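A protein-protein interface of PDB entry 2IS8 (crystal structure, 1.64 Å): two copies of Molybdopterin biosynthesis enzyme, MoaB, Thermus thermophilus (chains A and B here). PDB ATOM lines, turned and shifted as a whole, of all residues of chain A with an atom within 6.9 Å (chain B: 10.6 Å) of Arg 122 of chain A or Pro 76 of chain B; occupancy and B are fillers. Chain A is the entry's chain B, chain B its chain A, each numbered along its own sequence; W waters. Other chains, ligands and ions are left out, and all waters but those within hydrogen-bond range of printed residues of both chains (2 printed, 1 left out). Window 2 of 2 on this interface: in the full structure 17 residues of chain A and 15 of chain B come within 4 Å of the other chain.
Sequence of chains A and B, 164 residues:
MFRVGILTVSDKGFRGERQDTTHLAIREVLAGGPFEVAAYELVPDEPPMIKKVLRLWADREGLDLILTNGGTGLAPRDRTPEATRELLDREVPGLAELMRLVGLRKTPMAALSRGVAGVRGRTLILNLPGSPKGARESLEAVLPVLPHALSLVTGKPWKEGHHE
O of Leu 74 of chain B lies within hydrogen-bond range of NH2 of Arg 90 of chain A (3.3 Å).
Among the printed residues, merely in contact across the chains: Arg 122 of chain A with Pro 76 of chain B (3.5 Å), Leu 152 of chain A with Pro 76 of chain B (3.5 Å), Leu 152 of chain A with Ala 75 of chain B (3.7 Å), Val 153 of chain A with Leu 74 of chain B (3.8 Å), Leu 152 of chain A with Leu 74 of chain B (3.8 Å), Arg 90 of chain A with Arg 114 of chain B (3.9 Å) and Arg 90 of chain A with Glu 82 of chain B (3.96 Å).
Hydrophobic or aromatic side chains of chain B within 4 Å of the printed part of chain A: Leu 74 and Pro 76. Among the printed residues, no Asp or Glu carboxylate lies within 4 Å of a Lys or Arg side-chain nitrogen of the other chain.
The backbone carbonyl oxygen (O) of Gly 73 of chain B is in hydrogen-bond range of the guanidinium group (NE) of Arg 114 of chain B (3.0 Å). The backbone NH (N) of Ala 75 of chain B sits at hydrogen-bond distance from the side-chain carboxylate (OD2) of Asp 78 of chain B, 2.9 Å away. The backbone carbonyl oxygen (O) of Asp 78 of chain B is in hydrogen-bond range of the guanidinium group (NH2) of Arg 114 of chain B (2.7 Å). The side-chain carboxylate of Glu 82 of chain B is in salt-bridge range of the guanidinium group of Arg 114 of chain B. O of Arg 90 of chain A sits at hydrogen-bond distance from N of Val 119 of chain A, 2.8 Å away. The backbone carbonyl oxygen (O) of Val 153 of chain A sits at hydrogen-bond distance from the guanidinium group (NH1) of Arg 122 of chain A (2.9 Å).
Gly 62 of chain A touches none of the printed residues of chain B. No residue of chain B comes within 4 Å of Gly 121 of chain A. Of chain B, only Pro 76 comes within 4 Å of Arg 122 of chain A. No residue of chain B comes within 4 Å of Thr 123 of chain A. Val 153 of chain A touches just one residue of chain B: Leu 74. Of the printed residues of chain A, Leu 74 of chain B touches Arg 90 (3.3 Å), Leu 152 (3.8 Å) and Val 153 (3.8 Å). Pro 76 of chain B touches just these residues of chain A: Arg 122 (3.5 Å) and Leu 152 (3.5 Å). Printed residues of chain A within 4 Å of Glu 82 of chain B: Arg 90 (3.96 Å). The nearest residue of chain B that does not touch Arg 122 of chain A is Ala 75 of chain B (6.7 Å). The nearest residue of chain A that does not touch Pro 76 of chain B is Arg 90 of chain A (4.1 Å).
Water W1 bridges the backbone carbonyl oxygen of Asp 78 of chain B and the guanidinium group of Arg 90 of chain A. Water W2 lies within hydrogen-bond range of the backbone carbonyl oxygen (O) of Asp 89 of chain A (2.8 Å) and the side-chain carboxylate (OE2) of Glu 82 of chain B (3.4 Å).
No position is printed for both chains.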
ATOM      1  N   ALA A  58      10.137  42.342 -12.131  1.00  0.00           N
ATOM      2  CA  ALA A  58       9.680  41.346 -13.089  1.00  0.00           C
ATOM      3  C   ALA A  58       8.431  41.791 -13.837  1.00  0.00           C
ATOM      4  O   ALA A  58       8.427  41.869 -15.066  1.00  0.00           O
ATOM      5  CB  ALA A  58       9.410  40.025 -12.374  1.00  0.00           C
ATOM      6  N   GLY A  62      10.155  44.545 -16.241  1.00  0.00           N
ATOM      7  CA  GLY A  62      10.407  43.525 -17.241  1.00  0.00           C
ATOM      8  C   GLY A  62      11.848  43.075 -17.381  1.00  0.00           C
ATOM      9  O   GLY A  62      12.287  42.730 -18.479  1.00  0.00           O
ATOM     10  N   LEU A  63      12.590  43.065 -16.281  1.00  0.00           N
ATOM     11  CA  LEU A  63      13.982  42.632 -16.344  1.00  0.00           C
ATOM     12  C   LEU A  63      14.043  41.165 -16.761  1.00  0.00           C
ATOM     13  O   LEU A  63      13.121  40.389 -16.504  1.00  0.00           O
ATOM     14  CB  LEU A  63      14.668  42.820 -14.989  1.00  0.00           C
ATOM     15  CG  LEU A  63      14.778  44.256 -14.471  1.00  0.00           C
ATOM     16  CD1 LEU A  63      15.512  44.244 -13.150  1.00  0.00           C
ATOM     17  CD2 LEU A  63      15.513  45.131 -15.477  1.00  0.00           C
ATOM     18  N   ASP A  64      15.141  40.789 -17.404  1.00  0.00           N
ATOM     19  CA  ASP A  64      15.324  39.422 -17.871  1.00  0.00           C
ATOM     20  C   ASP A  64      15.898  38.524 -16.783  1.00  0.00           C
ATOM     21  O   ASP A  64      15.504  37.367 -16.645  1.00  0.00           O
ATOM     22  CB  ASP A  64      16.249  39.415 -19.086  1.00  0.00           C
ATOM     23  CG  ASP A  64      15.735  40.302 -20.203  1.00  0.00           C
ATOM     24  OD1 ASP A  64      14.527  40.210 -20.509  1.00  0.00           O
ATOM     25  OD2 ASP A  64      16.529  41.081 -20.776  1.00  0.00           O
ATOM     26  N   LEU A  65      16.826  39.073 -16.011  1.00  0.00           N
ATOM     27  CA  LEU A  65      17.477  38.322 -14.945  1.00  0.00           C
ATOM     28  C   LEU A  65      17.513  39.117 -13.655  1.00  0.00           C
ATOM     29  O   LEU A  65      17.822  40.308 -13.660  1.00  0.00           O
ATOM     30  CB  LEU A  65      18.919  37.976 -15.346  1.00  0.00           C
ATOM     31  CG  LEU A  65      19.776  37.293 -14.272  1.00  0.00           C
ATOM     32  CD1 LEU A  65      19.326  35.848 -14.087  1.00  0.00           C
ATOM     33  CD2 LEU A  65      21.250  37.348 -14.663  1.00  0.00           C
ATOM     34  N   ASP A  89       6.641  31.231 -10.618  1.00  0.00           N
ATOM     35  CA  ASP A  89       5.604  30.454 -11.287  1.00  0.00           C
ATOM     36  C   ASP A  89       6.090  29.014 -11.337  1.00  0.00           C
ATOM     37  O   ASP A  89       5.293  28.073 -11.298  1.00  0.00           O
ATOM     38  CB  ASP A  89       5.374  30.948 -12.717  1.00  0.00           C
ATOM     39  CG  ASP A  89       4.867  32.371 -12.777  1.00  0.00           C
ATOM     40  OD1 ASP A  89       4.112  32.783 -11.867  1.00  0.00           O
ATOM     41  OD2 ASP A  89       5.207  33.068 -13.753  1.00  0.00           O
ATOM     42  N   ARG A  90       7.410  28.858 -11.438  1.00  0.00           N
ATOM     43  CA  ARG A  90       8.050  27.547 -11.491  1.00  0.00           C
ATOM     44  C   ARG A  90       9.522  27.682 -11.114  1.00  0.00           C
ATOM     45  O   ARG A  90      10.118  28.745 -11.285  1.00  0.00           O
ATOM     46  CB  ARG A  90       7.915  26.933 -12.890  1.00  0.00           C
ATOM     47  CG  ARG A  90       8.525  27.746 -14.022  1.00  0.00           C
ATOM     48  CD  ARG A  90       8.231  27.100 -15.377  1.00  0.00           C
ATOM     49  NE  ARG A  90       8.842  27.823 -16.494  1.00  0.00           N
ATOM     50  CZ  ARG A  90       8.452  29.023 -16.923  1.00  0.00           C
ATOM     51  NH1 ARG A  90       7.443  29.648 -16.328  1.00  0.00           N
ATOM     52  NH2 ARG A  90       9.073  29.599 -17.948  1.00  0.00           N
ATOM     53  N   VAL A 119      11.407  31.019 -12.323  1.00  0.00           N
ATOM     54  CA  VAL A 119      10.899  31.977 -13.285  1.00  0.00           C
ATOM     55  C   VAL A 119       9.576  32.577 -12.830  1.00  0.00           C
ATOM     56  O   VAL A 119       8.747  31.887 -12.251  1.00  0.00           O
ATOM     57  CB  VAL A 119      10.666  31.307 -14.662  1.00  0.00           C
ATOM     58  CG1 VAL A 119      10.036  32.301 -15.633  1.00  0.00           C
ATOM     59  CG2 VAL A 119      11.992  30.777 -15.219  1.00  0.00           C
ATOM     60  N   ARG A 120       9.412  33.873 -13.074  1.00  0.00           N
ATOM     61  CA  ARG A 120       8.165  34.582 -12.801  1.00  0.00           C
ATOM     62  C   ARG A 120       7.935  35.343 -14.099  1.00  0.00           C
ATOM     63  O   ARG A 120       8.778  36.153 -14.505  1.00  0.00           O
ATOM     64  CB  ARG A 120       8.291  35.565 -11.631  1.00  0.00           C
ATOM     65  CG  ARG A 120       6.964  36.279 -11.326  1.00  0.00           C
ATOM     66  CD  ARG A 120       7.107  37.402 -10.309  1.00  0.00           C
ATOM     67  NE  ARG A 120       5.883  38.200 -10.199  1.00  0.00           N
ATOM     68  CZ  ARG A 120       4.788  37.824  -9.543  1.00  0.00           C
ATOM     69  NH1 ARG A 120       4.751  36.655  -8.916  1.00  0.00           N
ATOM     70  NH2 ARG A 120       3.722  38.617  -9.519  1.00  0.00           N
ATOM     71  N   GLY A 121       6.815  35.075 -14.767  1.00  0.00           N
ATOM     72  CA  GLY A 121       6.544  35.737 -16.036  1.00  0.00           C
ATOM     73  C   GLY A 121       7.660  35.396 -17.009  1.00  0.00           C
ATOM     74  O   GLY A 121       7.837  34.232 -17.358  1.00  0.00           O
ATOM     75  N   ARG A 122       8.418  36.399 -17.441  1.00  0.00           N
ATOM     76  CA  ARG A 122       9.533  36.171 -18.350  1.00  0.00           C
ATOM     77  C   ARG A 122      10.835  36.644 -17.709  1.00  0.00           C
ATOM     78  O   ARG A 122      11.727  37.150 -18.387  1.00  0.00           O
ATOM     79  CB  ARG A 122       9.307  36.888 -19.684  1.00  0.00           C
ATOM     80  CG  ARG A 122       8.309  36.168 -20.586  1.00  0.00           C
ATOM     81  CD  ARG A 122       8.197  36.832 -21.946  1.00  0.00           C
ATOM     82  NE  ARG A 122       7.413  36.028 -22.881  1.00  0.00           N
ATOM     83  CZ  ARG A 122       7.768  34.822 -23.316  1.00  0.00           C
ATOM     84  NH1 ARG A 122       8.901  34.268 -22.902  1.00  0.00           N
ATOM     85  NH2 ARG A 122       6.991  34.170 -24.168  1.00  0.00           N
ATOM     86  N   THR A 123      10.925  36.464 -16.395  1.00  0.00           N
ATOM     87  CA  THR A 123      12.098  36.862 -15.634  1.00  0.00           C
ATOM     88  C   THR A 123      12.684  35.678 -14.876  1.00  0.00           C
ATOM     89  O   THR A 123      11.970  34.964 -14.176  1.00  0.00           O
ATOM     90  CB  THR A 123      11.751  37.976 -14.617  1.00  0.00           C
ATOM     91  OG1 THR A 123      11.186  39.095 -15.313  1.00  0.00           O
ATOM     92  CG2 THR A 123      13.001  38.431 -13.870  1.00  0.00           C
ATOM     93  N   LEU A 124      13.986  35.462 -15.042  1.00  0.00           N
ATOM     94  CA  LEU A 124      14.677  34.392 -14.335  1.00  0.00           C
ATOM     95  C   LEU A 124      15.241  35.019 -13.073  1.00  0.00           C
ATOM     96  O   LEU A 124      15.870  36.071 -13.130  1.00  0.00           O
ATOM     97  CB  LEU A 124      15.810  33.830 -15.198  1.00  0.00           C
ATOM     98  CG  LEU A 124      16.683  32.715 -14.612  1.00  0.00           C
ATOM     99  CD1 LEU A 124      15.856  31.466 -14.299  1.00  0.00           C
ATOM    100  CD2 LEU A 124      17.775  32.390 -15.616  1.00  0.00           C
ATOM    101  N   LEU A 150      18.451  32.220 -20.249  1.00  0.00           N
ATOM    102  CA  LEU A 150      17.708  33.460 -20.450  1.00  0.00           C
ATOM    103  C   LEU A 150      17.022  33.533 -21.811  1.00  0.00           C
ATOM    104  O   LEU A 150      15.906  34.039 -21.909  1.00  0.00           O
ATOM    105  CB  LEU A 150      18.636  34.673 -20.255  1.00  0.00           C
ATOM    106  CG  LEU A 150      19.013  34.890 -18.786  1.00  0.00           C
ATOM    107  CD1 LEU A 150      20.242  35.780 -18.681  1.00  0.00           C
ATOM    108  CD2 LEU A 150      17.832  35.501 -18.038  1.00  0.00           C
ATOM    109  N   SER A 151      17.670  33.026 -22.857  1.00  0.00           N
ATOM    110  CA  SER A 151      17.058  33.073 -24.185  1.00  0.00           C
ATOM    111  C   SER A 151      15.730  32.312 -24.184  1.00  0.00           C
ATOM    112  O   SER A 151      14.750  32.749 -24.790  1.00  0.00           O
ATOM    113  CB  SER A 151      18.008  32.505 -25.257  1.00  0.00           C
ATOM    114  OG  SER A 151      18.260  31.123 -25.078  1.00  0.00           O
ATOM    115  N   LEU A 152      15.692  31.190 -23.470  1.00  0.00           N
ATOM    116  CA  LEU A 152      14.483  30.378 -23.389  1.00  0.00           C
ATOM    117  C   LEU A 152      13.391  31.027 -22.538  1.00  0.00           C
ATOM    118  O   LEU A 152      12.216  31.022 -22.904  1.00  0.00           O
ATOM    119  CB  LEU A 152      14.819  28.996 -22.823  1.00  0.00           C
ATOM    120  CG  LEU A 152      15.690  28.105 -23.716  1.00  0.00           C
ATOM    121  CD1 LEU A 152      15.993  26.794 -22.999  1.00  0.00           C
ATOM    122  CD2 LEU A 152      14.972  27.842 -25.038  1.00  0.00           C
ATOM    123  N   VAL A 153      13.781  31.592 -21.404  1.00  0.00           N
ATOM    124  CA  VAL A 153      12.826  32.238 -20.511  1.00  0.00           C
ATOM    125  C   VAL A 153      12.246  33.520 -21.088  1.00  0.00           C
ATOM    126  O   VAL A 153      11.041  33.771 -20.993  1.00  0.00           O
ATOM    127  CB  VAL A 153      13.490  32.591 -19.161  1.00  0.00           C
ATOM    128  CG1 VAL A 153      12.573  33.485 -18.335  1.00  0.00           C
ATOM    129  CG2 VAL A 153      13.821  31.326 -18.403  1.00  0.00           C
ATOM    130  N   THR A 154      13.113  34.331 -21.683  1.00  0.00           N
ATOM    131  CA  THR A 154      12.718  35.627 -22.221  1.00  0.00           C
ATOM    132  C   THR A 154      12.327  35.634 -23.688  1.00  0.00           C
ATOM    133  O   THR A 154      11.655  36.558 -24.151  1.00  0.00           O
ATOM    134  CB  THR A 154      13.851  36.644 -22.052  1.00  0.00           C
ATOM    135  OG1 THR A 154      14.938  36.283 -22.916  1.00  0.00           O
ATOM    136  CG2 THR A 154      14.343  36.654 -20.616  1.00  0.00           C
ATOM    137  N   GLY A 155      12.770  34.618 -24.417  1.00  0.00           N
ATOM    138  CA  GLY A 155      12.475  34.542 -25.834  1.00  0.00           C
ATOM    139  C   GLY A 155      13.351  35.495 -26.626  1.00  0.00           C
ATOM    140  O   GLY A 155      13.141  35.687 -27.826  1.00  0.00           O
ATOM    141  N   LYS A 156      14.334  36.094 -25.957  1.00  0.00           N
ATOM    142  CA  LYS A 156      15.239  37.044 -26.600  1.00  0.00           C
ATOM    143  C   LYS A 156      16.545  36.389 -27.039  1.00  0.00           C
ATOM    144  O   LYS A 156      17.029  35.451 -26.404  1.00  0.00           O
ATOM    145  CB  LYS A 156      15.556  38.203 -25.657  1.00  0.00           C
ATOM    146  CG  LYS A 156      14.334  38.967 -25.196  1.00  0.00           C
ATOM    147  CD  LYS A 156      14.707  40.048 -24.203  1.00  0.00           C
ATOM    148  CE  LYS A 156      13.465  40.697 -23.638  1.00  0.00           C
ATOM    149  NZ  LYS A 156      13.811  41.830 -22.752  1.00  0.00           N
ATOM    150  N   ASP B  11       5.965  19.514 -29.590  1.00  0.00           N
ATOM    151  CA  ASP B  11       5.017  20.194 -30.468  1.00  0.00           C
ATOM    152  C   ASP B  11       5.378  19.880 -31.927  1.00  0.00           C
ATOM    153  O   ASP B  11       4.523  19.478 -32.712  1.00  0.00           O
ATOM    154  CB  ASP B  11       5.044  21.721 -30.268  1.00  0.00           C
ATOM    155  CG  ASP B  11       4.292  22.182 -29.019  1.00  0.00           C
ATOM    156  OD1 ASP B  11       3.342  21.500 -28.584  1.00  0.00           O
ATOM    157  OD2 ASP B  11       4.643  23.257 -28.480  1.00  0.00           O
ATOM    158  N   ASP B  45       3.177  19.789 -26.299  1.00  0.00           N
ATOM    159  CA  ASP B  45       3.397  20.386 -24.981  1.00  0.00           C
ATOM    160  C   ASP B  45       2.058  20.802 -24.375  1.00  0.00           C
ATOM    161  O   ASP B  45       1.828  21.982 -24.112  1.00  0.00           O
ATOM    162  CB  ASP B  45       4.302  21.621 -25.088  1.00  0.00           C
ATOM    163  CG  ASP B  45       5.732  21.281 -25.474  1.00  0.00           C
ATOM    164  OD1 ASP B  45       6.345  20.404 -24.828  1.00  0.00           O
ATOM    165  OD2 ASP B  45       6.250  21.915 -26.415  1.00  0.00           O
ATOM    166  N   GLU B  46       1.185  19.826 -24.162  1.00  0.00           N
ATOM    167  CA  GLU B  46      -0.138  20.075 -23.595  1.00  0.00           C
ATOM    168  C   GLU B  46      -0.324  19.182 -22.371  1.00  0.00           C
ATOM    169  O   GLU B  46      -0.455  17.963 -22.486  1.00  0.00           O
ATOM    170  CB  GLU B  46      -1.226  19.779 -24.636  1.00  0.00           C
ATOM    171  CG  GLU B  46      -1.270  20.745 -25.831  1.00  0.00           C
ATOM    172  CD  GLU B  46      -1.625  22.176 -25.433  1.00  0.00           C
ATOM    173  OE1 GLU B  46      -2.269  22.365 -24.384  1.00  0.00           O
ATOM    174  OE2 GLU B  46      -1.273  23.117 -26.175  1.00  0.00           O
ATOM    175  N   PRO B  47      -0.332  19.788 -21.172  1.00  0.00           N
ATOM    176  CA  PRO B  47      -0.497  19.033 -19.929  1.00  0.00           C
ATOM    177  C   PRO B  47      -1.592  17.957 -19.928  1.00  0.00           C
ATOM    178  O   PRO B  47      -1.354  16.836 -19.491  1.00  0.00           O
ATOM    179  CB  PRO B  47      -0.728  20.137 -18.891  1.00  0.00           C
ATOM    180  CG  PRO B  47       0.167  21.239 -19.412  1.00  0.00           C
ATOM    181  CD  PRO B  47      -0.149  21.225 -20.902  1.00  0.00           C
ATOM    182  N   ILE B  50      -0.440  14.956 -21.914  1.00  0.00           N
ATOM    183  CA  ILE B  50       0.666  14.287 -21.241  1.00  0.00           C
ATOM    184  C   ILE B  50       0.103  13.454 -20.091  1.00  0.00           C
ATOM    185  O   ILE B  50       0.405  12.270 -19.958  1.00  0.00           O
ATOM    186  CB  ILE B  50       1.670  15.320 -20.677  1.00  0.00           C
ATOM    187  CG1 ILE B  50       2.276  16.128 -21.821  1.00  0.00           C
ATOM    188  CG2 ILE B  50       2.757  14.609 -19.856  1.00  0.00           C
ATOM    189  CD1 ILE B  50       3.057  17.342 -21.355  1.00  0.00           C
ATOM    190  N   GLY B  71      10.005  18.733 -23.232  1.00  0.00           N
ATOM    191  CA  GLY B  71       9.200  19.626 -22.418  1.00  0.00           C
ATOM    192  C   GLY B  71       9.657  19.862 -20.990  1.00  0.00           C
ATOM    193  O   GLY B  71       8.842  20.223 -20.140  1.00  0.00           O
ATOM    194  N   THR B  72      10.947  19.690 -20.709  1.00  0.00           N
ATOM    195  CA  THR B  72      11.437  19.907 -19.349  1.00  0.00           C
ATOM    196  C   THR B  72      12.277  21.173 -19.218  1.00  0.00           C
ATOM    197  O   THR B  72      12.757  21.491 -18.126  1.00  0.00           O
ATOM    198  CB  THR B  72      12.306  18.735 -18.856  1.00  0.00           C
ATOM    199  OG1 THR B  72      13.490  18.656 -19.658  1.00  0.00           O
ATOM    200  CG2 THR B  72      11.540  17.419 -18.943  1.00  0.00           C
ATOM    201  N   GLY B  73      12.442  21.883 -20.327  1.00  0.00           N
ATOM    202  CA  GLY B  73      13.251  23.091 -20.341  1.00  0.00           C
ATOM    203  C   GLY B  73      12.625  24.330 -19.729  1.00  0.00           C
ATOM    204  O   GLY B  73      11.594  24.261 -19.061  1.00  0.00           O
ATOM    205  N   LEU B  74      13.262  25.473 -19.976  1.00  0.00           N
ATOM    206  CA  LEU B  74      12.823  26.749 -19.428  1.00  0.00           C
ATOM    207  C   LEU B  74      11.898  27.558 -20.327  1.00  0.00           C
ATOM    208  O   LEU B  74      11.492  28.664 -19.961  1.00  0.00           O
ATOM    209  CB  LEU B  74      14.048  27.591 -19.048  1.00  0.00           C
ATOM    210  CG  LEU B  74      14.660  27.291 -17.673  1.00  0.00           C
ATOM    211  CD1 LEU B  74      14.928  25.815 -17.517  1.00  0.00           C
ATOM    212  CD2 LEU B  74      15.942  28.085 -17.500  1.00  0.00           C
ATOM    213  N   ALA B  75      11.568  27.015 -21.496  1.00  0.00           N
ATOM    214  CA  ALA B  75      10.658  27.689 -22.424  1.00  0.00           C
ATOM    215  C   ALA B  75       9.266  27.703 -21.794  1.00  0.00           C
ATOM    216  O   ALA B  75       8.895  26.785 -21.061  1.00  0.00           O
ATOM    217  CB  ALA B  75      10.628  26.960 -23.756  1.00  0.00           C
ATOM    218  N   PRO B  76       8.478  28.752 -22.068  1.00  0.00           N
ATOM    219  CA  PRO B  76       7.127  28.866 -21.511  1.00  0.00           C
ATOM    220  C   PRO B  76       6.216  27.655 -21.736  1.00  0.00           C
ATOM    221  O   PRO B  76       5.400  27.322 -20.876  1.00  0.00           O
ATOM    222  CB  PRO B  76       6.594  30.131 -22.177  1.00  0.00           C
ATOM    223  CG  PRO B  76       7.835  30.966 -22.319  1.00  0.00           C
ATOM    224  CD  PRO B  76       8.836  29.959 -22.836  1.00  0.00           C
ATOM    225  N   ARG B  77       6.359  26.998 -22.885  1.00  0.00           N
ATOM    226  CA  ARG B  77       5.532  25.837 -23.213  1.00  0.00           C
ATOM    227  C   ARG B  77       5.973  24.532 -22.535  1.00  0.00           C
ATOM    228  O   ARG B  77       5.200  23.570 -22.484  1.00  0.00           O
ATOM    229  CB  ARG B  77       5.499  25.623 -24.731  1.00  0.00           C
ATOM    230  CG  ARG B  77       4.769  26.717 -25.518  1.00  0.00           C
ATOM    231  CD  ARG B  77       3.258  26.501 -25.538  1.00  0.00           C
ATOM    232  NE  ARG B  77       2.883  25.293 -26.271  1.00  0.00           N
ATOM    233  CZ  ARG B  77       1.644  24.808 -26.329  1.00  0.00           C
ATOM    234  NH1 ARG B  77       0.658  25.430 -25.698  1.00  0.00           N
ATOM    235  NH2 ARG B  77       1.392  23.691 -27.001  1.00  0.00           N
ATOM    236  N   ASP B  78       7.199  24.495 -22.019  1.00  0.00           N
ATOM    237  CA  ASP B  78       7.703  23.287 -21.367  1.00  0.00           C
ATOM    238  C   ASP B  78       6.990  23.065 -20.045  1.00  0.00           C
ATOM    239  O   ASP B  78       7.298  23.720 -19.056  1.00  0.00           O
ATOM    240  CB  ASP B  78       9.213  23.394 -21.112  1.00  0.00           C
ATOM    241  CG  ASP B  78      10.009  23.536 -22.383  1.00  0.00           C
ATOM    242  OD1 ASP B  78       9.648  22.881 -23.381  1.00  0.00           O
ATOM    243  OD2 ASP B  78      11.005  24.295 -22.376  1.00  0.00           O
ATOM    244  N   ARG B  79       6.046  22.131 -20.027  1.00  0.00           N
ATOM    245  CA  ARG B  79       5.287  21.855 -18.811  1.00  0.00           C
ATOM    246  C   ARG B  79       5.225  20.378 -18.433  1.00  0.00           C
ATOM    247  O   ARG B  79       4.369  19.973 -17.651  1.00  0.00           O
ATOM    248  CB  ARG B  79       3.870  22.416 -18.961  1.00  0.00           C
ATOM    249  CG  ARG B  79       3.830  23.934 -19.002  1.00  0.00           C
ATOM    250  CD  ARG B  79       2.457  24.451 -19.371  1.00  0.00           C
ATOM    251  NE  ARG B  79       2.175  24.245 -20.787  1.00  0.00           N
ATOM    252  CZ  ARG B  79       1.046  24.609 -21.382  1.00  0.00           C
ATOM    253  NH1 ARG B  79       0.089  25.197 -20.683  1.00  0.00           N
ATOM    254  NH2 ARG B  79       0.879  24.390 -22.680  1.00  0.00           N
ATOM    255  N   THR B  80       6.129  19.569 -18.978  1.00  0.00           N
ATOM    256  CA  THR B  80       6.137  18.153 -18.648  1.00  0.00           C
ATOM    257  C   THR B  80       6.361  17.907 -17.151  1.00  0.00           C
ATOM    258  O   THR B  80       5.702  17.055 -16.559  1.00  0.00           O
ATOM    259  CB  THR B  80       7.205  17.394 -19.479  1.00  0.00           C
ATOM    260  OG1 THR B  80       6.912  17.557 -20.872  1.00  0.00           O
ATOM    261  CG2 THR B  80       7.199  15.913 -19.144  1.00  0.00           C
ATOM    262  N   PRO B  81       7.280  18.663 -16.513  1.00  0.00           N
ATOM    263  CA  PRO B  81       7.536  18.470 -15.081  1.00  0.00           C
ATOM    264  C   PRO B  81       6.289  18.677 -14.231  1.00  0.00           C
ATOM    265  O   PRO B  81       5.955  17.835 -13.401  1.00  0.00           O
ATOM    266  CB  PRO B  81       8.617  19.509 -14.775  1.00  0.00           C
ATOM    267  CG  PRO B  81       9.351  19.619 -16.074  1.00  0.00           C
ATOM    268  CD  PRO B  81       8.217  19.648 -17.080  1.00  0.00           C
ATOM    269  N   GLU B  82       5.614  19.804 -14.441  1.00  0.00           N
ATOM    270  CA  GLU B  82       4.389  20.116 -13.702  1.00  0.00           C
ATOM    271  C   GLU B  82       3.340  19.034 -13.928  1.00  0.00           C
ATOM    272  O   GLU B  82       2.776  18.490 -12.980  1.00  0.00           O
ATOM    273  CB  GLU B  82       3.800  21.449 -14.172  1.00  0.00           C
ATOM    274  CG  GLU B  82       4.543  22.699 -13.743  1.00  0.00           C
ATOM    275  CD  GLU B  82       5.957  22.782 -14.285  1.00  0.00           C
ATOM    276  OE1 GLU B  82       6.171  22.479 -15.479  1.00  0.00           O
ATOM    277  OE2 GLU B  82       6.855  23.170 -13.508  1.00  0.00           O
ATOM    278  N   ALA B  83       3.066  18.745 -15.194  1.00  0.00           N
ATOM    279  CA  ALA B  83       2.067  17.745 -15.555  1.00  0.00           C
ATOM    280  C   ALA B  83       2.352  16.395 -14.899  1.00  0.00           C
ATOM    281  O   ALA B  83       1.435  15.683 -14.479  1.00  0.00           O
ATOM    282  CB  ALA B  83       2.011  17.598 -17.079  1.00  0.00           C
ATOM    283  N   LEU B 112      19.716  22.674 -17.006  1.00  0.00           N
ATOM    284  CA  LEU B 112      18.528  23.445 -17.352  1.00  0.00           C
ATOM    285  C   LEU B 112      17.294  22.576 -17.549  1.00  0.00           C
ATOM    286  O   LEU B 112      16.273  23.046 -18.049  1.00  0.00           O
ATOM    287  CB  LEU B 112      18.772  24.277 -18.608  1.00  0.00           C
ATOM    288  CG  LEU B 112      19.918  25.286 -18.506  1.00  0.00           C
ATOM    289  CD1 LEU B 112      19.977  26.089 -19.794  1.00  0.00           C
ATOM    290  CD2 LEU B 112      19.708  26.207 -17.305  1.00  0.00           C
ATOM    291  N   ARG B 114      14.177  20.679 -15.973  1.00  0.00           N
ATOM    292  CA  ARG B 114      13.376  20.705 -14.759  1.00  0.00           C
ATOM    293  C   ARG B 114      12.662  19.373 -14.554  1.00  0.00           C
ATOM    294  O   ARG B 114      11.789  19.253 -13.700  1.00  0.00           O
ATOM    295  CB  ARG B 114      12.345  21.834 -14.838  1.00  0.00           C
ATOM    296  CG  ARG B 114      12.957  23.206 -15.056  1.00  0.00           C
ATOM    297  CD  ARG B 114      11.885  24.280 -15.139  1.00  0.00           C
ATOM    298  NE  ARG B 114      10.892  23.989 -16.171  1.00  0.00           N
ATOM    299  CZ  ARG B 114       9.670  23.526 -15.919  1.00  0.00           C
ATOM    300  NH1 ARG B 114       9.286  23.299 -14.671  1.00  0.00           N
ATOM    301  NH2 ARG B 114       8.825  23.304 -16.914  1.00  0.00           N
HETATM  302  O   HOH W   1       6.617  25.971 -17.811  1.00  0.00           O
HETATM  303  O   HOH W   2       4.943  25.367 -11.798  1.00  0.00           O
